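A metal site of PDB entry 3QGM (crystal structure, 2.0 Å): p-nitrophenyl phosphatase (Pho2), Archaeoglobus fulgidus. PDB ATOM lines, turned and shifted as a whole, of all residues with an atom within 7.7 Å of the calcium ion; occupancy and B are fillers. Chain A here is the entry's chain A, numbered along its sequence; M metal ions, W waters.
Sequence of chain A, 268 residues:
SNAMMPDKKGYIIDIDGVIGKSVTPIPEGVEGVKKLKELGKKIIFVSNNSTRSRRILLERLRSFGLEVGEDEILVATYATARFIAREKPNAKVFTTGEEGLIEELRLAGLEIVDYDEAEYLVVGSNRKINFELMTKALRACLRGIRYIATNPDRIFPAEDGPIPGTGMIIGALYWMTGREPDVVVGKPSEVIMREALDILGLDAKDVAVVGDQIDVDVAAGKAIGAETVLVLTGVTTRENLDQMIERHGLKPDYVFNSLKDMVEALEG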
ATOM      1  N   ASP A  14       3.140  27.820  -0.401  1.00  0.00           N
ATOM      2  CA  ASP A  14       1.997  28.781  -0.471  1.00  0.00           C
ATOM      3  C   ASP A  14       2.541  30.191  -0.173  1.00  0.00           C
ATOM      4  O   ASP A  14       3.419  30.356   0.693  1.00  0.00           O
ATOM      5  CB  ASP A  14       0.959  28.280   0.529  1.00  0.00           C
ATOM      6  CG  ASP A  14      -0.159  29.268   0.866  1.00  0.00           C
ATOM      7  OD1 ASP A  14      -0.732  30.030   0.035  1.00  0.00           O
ATOM      8  OD2 ASP A  14      -0.484  29.213   2.063  1.00  0.00           O
ATOM      9  N   ILE A  15       2.062  31.192  -0.905  1.00  0.00           N
ATOM     10  CA  ILE A  15       2.501  32.578  -0.716  1.00  0.00           C
ATOM     11  C   ILE A  15       1.664  33.245   0.388  1.00  0.00           C
ATOM     12  O   ILE A  15       2.221  33.628   1.424  1.00  0.00           O
ATOM     13  CB  ILE A  15       2.363  33.385  -2.010  1.00  0.00           C
ATOM     14  CG1 ILE A  15       3.283  32.803  -3.107  1.00  0.00           C
ATOM     15  CG2 ILE A  15       2.701  34.880  -1.787  1.00  0.00           C
ATOM     16  CD1 ILE A  15       3.005  33.374  -4.496  1.00  0.00           C
ATOM     17  N   ASP A  16       0.366  33.378   0.191  1.00  0.00           N
ATOM     18  CA  ASP A  16      -0.467  34.141   1.163  1.00  0.00           C
ATOM     19  C   ASP A  16      -0.675  33.423   2.485  1.00  0.00           C
ATOM     20  O   ASP A  16      -1.181  32.287   2.548  1.00  0.00           O
ATOM     21  CB  ASP A  16      -1.816  34.593   0.556  1.00  0.00           C
ATOM     22  CG  ASP A  16      -2.134  36.066   0.884  1.00  0.00           C
ATOM     23  OD1 ASP A  16      -1.407  36.968   0.351  1.00  0.00           O
ATOM     24  OD2 ASP A  16      -3.073  36.311   1.690  1.00  0.00           O
ATOM     25  N   GLY A  17      -0.256  34.093   3.549  1.00  0.00           N
ATOM     26  CA  GLY A  17      -0.317  33.568   4.926  1.00  0.00           C
ATOM     27  C   GLY A  17       1.022  32.979   5.309  1.00  0.00           C
ATOM     28  O   GLY A  17       1.242  32.568   6.453  1.00  0.00           O
ATOM     29  N   VAL A  18       1.949  32.922   4.343  1.00  0.00           N
ATOM     30  CA  VAL A  18       3.241  32.264   4.581  1.00  0.00           C
ATOM     31  C   VAL A  18       4.366  33.265   4.348  1.00  0.00           C
ATOM     32  O   VAL A  18       5.166  33.503   5.256  1.00  0.00           O
ATOM     33  CB  VAL A  18       3.461  31.025   3.664  1.00  0.00           C
ATOM     34  CG1 VAL A  18       4.857  30.338   3.991  1.00  0.00           C
ATOM     35  CG2 VAL A  18       2.314  30.069   3.762  1.00  0.00           C
ATOM     36  N   GLY A  20       3.712  36.512   2.489  1.00  0.00           N
ATOM     37  CA  GLY A  20       3.119  37.803   2.597  1.00  0.00           C
ATOM     38  C   GLY A  20       1.639  37.713   2.861  1.00  0.00           C
ATOM     39  O   GLY A  20       1.033  36.640   2.810  1.00  0.00           O
ATOM     40  N   VAL A  46       3.445  28.554  -4.946  1.00  0.00           N
ATOM     41  CA  VAL A  46       2.222  28.122  -5.626  1.00  0.00           C
ATOM     42  C   VAL A  46       1.046  28.873  -5.029  1.00  0.00           C
ATOM     43  O   VAL A  46       0.885  28.863  -3.818  1.00  0.00           O
ATOM     44  CB  VAL A  46       2.004  26.597  -5.560  1.00  0.00           C
ATOM     45  CG1 VAL A  46       0.634  26.199  -6.128  1.00  0.00           C
ATOM     46  CG2 VAL A  46       3.090  25.827  -6.339  1.00  0.00           C
ATOM     47  N   SER A  47       0.247  29.532  -5.865  1.00  0.00           N
ATOM     48  CA  SER A  47      -0.871  30.318  -5.379  1.00  0.00           C
ATOM     49  C   SER A  47      -2.112  30.087  -6.196  1.00  0.00           C
ATOM     50  O   SER A  47      -2.032  29.928  -7.400  1.00  0.00           O
ATOM     51  CB  SER A  47      -0.553  31.818  -5.491  1.00  0.00           C
ATOM     52  OG  SER A  47      -1.713  32.577  -5.278  1.00  0.00           O
ATOM     53  N   ASN A  48      -3.267  30.077  -5.516  1.00  0.00           N
ATOM     54  CA  ASN A  48      -4.538  29.904  -6.157  1.00  0.00           C
ATOM     55  C   ASN A  48      -5.094  31.188  -6.690  1.00  0.00           C
ATOM     56  O   ASN A  48      -6.213  31.186  -7.174  1.00  0.00           O
ATOM     57  CB  ASN A  48      -5.543  29.302  -5.185  1.00  0.00           C
ATOM     58  CG  ASN A  48      -5.476  27.791  -5.151  1.00  0.00           C
ATOM     59  OD1 ASN A  48      -4.609  27.186  -5.774  1.00  0.00           O
ATOM     60  ND2 ASN A  48      -6.448  27.165  -4.453  1.00  0.00           N
ATOM     61  N   LYS A 187      -5.095  24.454  -5.929  1.00  0.00           N
ATOM     62  CA  LYS A 187      -5.116  23.644  -4.727  1.00  0.00           C
ATOM     63  C   LYS A 187      -6.523  23.487  -4.133  1.00  0.00           C
ATOM     64  O   LYS A 187      -7.237  24.490  -4.005  1.00  0.00           O
ATOM     65  CB  LYS A 187      -4.190  24.236  -3.652  1.00  0.00           C
ATOM     66  CG  LYS A 187      -2.659  24.279  -4.083  1.00  0.00           C
ATOM     67  CD  LYS A 187      -1.833  25.004  -3.020  1.00  0.00           C
ATOM     68  CE  LYS A 187      -2.085  26.491  -2.986  1.00  0.00           C
ATOM     69  NZ  LYS A 187      -1.303  27.134  -1.906  1.00  0.00           N
ATOM     70  N   VAL A 210       4.170  23.440   1.903  1.00  0.00           N
ATOM     71  CA  VAL A 210       4.067  24.297   3.083  1.00  0.00           C
ATOM     72  C   VAL A 210       2.963  25.275   2.808  1.00  0.00           C
ATOM     73  O   VAL A 210       2.880  25.819   1.682  1.00  0.00           O
ATOM     74  CB  VAL A 210       5.337  25.147   3.282  1.00  0.00           C
ATOM     75  CG1 VAL A 210       5.185  26.044   4.543  1.00  0.00           C
ATOM     76  CG2 VAL A 210       6.598  24.264   3.412  1.00  0.00           C
ATOM     77  N   GLY A 211       2.152  25.525   3.836  1.00  0.00           N
ATOM     78  CA  GLY A 211       1.030  26.410   3.738  1.00  0.00           C
ATOM     79  C   GLY A 211       0.349  26.705   5.050  1.00  0.00           C
ATOM     80  O   GLY A 211       0.745  26.211   6.115  1.00  0.00           O
ATOM     81  N   ASP A 212      -0.694  27.516   4.959  1.00  0.00           N
ATOM     82  CA  ASP A 212      -1.392  28.021   6.132  1.00  0.00           C
ATOM     83  C   ASP A 212      -2.787  27.465   6.271  1.00  0.00           C
ATOM     84  O   ASP A 212      -3.409  27.771   7.256  1.00  0.00           O
ATOM     85  CB  ASP A 212      -1.412  29.570   6.179  1.00  0.00           C
ATOM     86  CG  ASP A 212      -2.346  30.181   5.124  1.00  0.00           C
ATOM     87  OD1 ASP A 212      -2.510  29.606   4.036  1.00  0.00           O
ATOM     88  OD2 ASP A 212      -2.885  31.264   5.397  1.00  0.00           O
ATOM     89  N   GLN A 213      -3.248  26.667   5.298  1.00  0.00           N
ATOM     90  CA  GLN A 213      -4.594  26.070   5.306  1.00  0.00           C
ATOM     91  C   GLN A 213      -4.584  24.541   5.174  1.00  0.00           C
ATOM     92  O   GLN A 213      -4.068  23.968   4.192  1.00  0.00           O
ATOM     93  CB  GLN A 213      -5.442  26.659   4.178  1.00  0.00           C
ATOM     94  CG  GLN A 213      -5.740  28.126   4.334  1.00  0.00           C
ATOM     95  CD  GLN A 213      -6.731  28.641   3.285  1.00  0.00           C
ATOM     96  OE1 GLN A 213      -7.881  28.898   3.596  1.00  0.00           O
ATOM     97  NE2 GLN A 213      -6.267  28.822   2.070  1.00  0.00           N
ATOM     98  N   VAL A 216      -6.552  23.319   2.185  1.00  0.00           N
ATOM     99  CA  VAL A 216      -6.014  23.682   0.890  1.00  0.00           C
ATOM    100  C   VAL A 216      -4.623  23.085   0.734  1.00  0.00           C
ATOM    101  O   VAL A 216      -4.365  22.221  -0.137  1.00  0.00           O
ATOM    102  CB  VAL A 216      -6.028  25.224   0.761  1.00  0.00           C
ATOM    103  CG1 VAL A 216      -5.331  25.684  -0.508  1.00  0.00           C
ATOM    104  CG2 VAL A 216      -7.527  25.748   0.824  1.00  0.00           C
ATOM    105  N   ASP A 217      -3.722  23.532   1.586  1.00  0.00           N
ATOM    106  CA  ASP A 217      -2.311  23.209   1.444  1.00  0.00           C
ATOM    107  C   ASP A 217      -1.988  21.793   1.911  1.00  0.00           C
ATOM    108  O   ASP A 217      -1.291  21.070   1.214  1.00  0.00           O
ATOM    109  CB  ASP A 217      -1.509  24.241   2.207  1.00  0.00           C
ATOM    110  CG  ASP A 217      -1.801  25.632   1.728  1.00  0.00           C
ATOM    111  OD1 ASP A 217      -1.439  25.867   0.550  1.00  0.00           O
ATOM    112  OD2 ASP A 217      -2.486  26.423   2.457  1.00  0.00           O
ATOM    113  N   GLY A 234      -0.748  32.519   9.143  1.00  0.00           N
ATOM    114  CA  GLY A 234      -1.881  32.907   8.301  1.00  0.00           C
ATOM    115  C   GLY A 234      -3.200  32.393   8.859  1.00  0.00           C
ATOM    116  O   GLY A 234      -3.440  32.541  10.049  1.00  0.00           O
ATOM    117  N   VAL A 235      -4.028  31.777   8.024  1.00  0.00           N
ATOM    118  CA  VAL A 235      -5.388  31.345   8.399  1.00  0.00           C
ATOM    119  C   VAL A 235      -5.424  30.404   9.676  1.00  0.00           C
ATOM    120  O   VAL A 235      -6.333  30.500  10.519  1.00  0.00           O
ATOM    121  CB  VAL A 235      -6.093  30.684   7.175  1.00  0.00           C
ATOM    122  CG1 VAL A 235      -7.346  29.951   7.546  1.00  0.00           C
ATOM    123  CG2 VAL A 235      -6.373  31.721   6.028  1.00  0.00           C
HETATM  124 CA    CA M   1      -2.479  30.505   1.947  1.00  0.00          CA
HETATM  125  O   HOH W   1      -4.086  31.892   3.153  1.00  0.00           O
HETATM  126  O   HOH W   2      -3.503  28.732   1.323  1.00  0.00           O
HETATM  127  O   HOH W   3      -3.582  31.528   0.137  1.00  0.00           O
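Of the 18 residues printed, 3 come within 4 Å of the calcium ion.
N of Asp 212 sits at hydrogen-bond distance from OD2 of Asp 217.
OD2 of Asp 212 sits at hydrogen-bond distance from N of Val 235 (2.9 Å).
The side-chain amino group (NZ) of Lys 187 sits close to the side-chain carboxylate (OD1) of Asp 14.
O of Val 210 is in hydrogen-bond range of N of Asp 14 (2.9 Å).
The calcium ion is bound by water W2 (2.1 Å), the side-chain carboxylate (OD1) of Asp 212 (2.3 Å), the backbone carbonyl oxygen (O) of Asp 16 (2.3 Å), water W3 (2.4 Å), the side-chain carboxylate (OD2) of Asp 14 (2.4 Å), water W1 (2.4 Å) and the side-chain carboxylate (OD1) of Asp 14 (2.6 Å).
Water W2 lies within hydrogen-bond range of OD2 of Asp 217 (2.8 Å) and NE2 of Gln 213 (2.9 Å).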
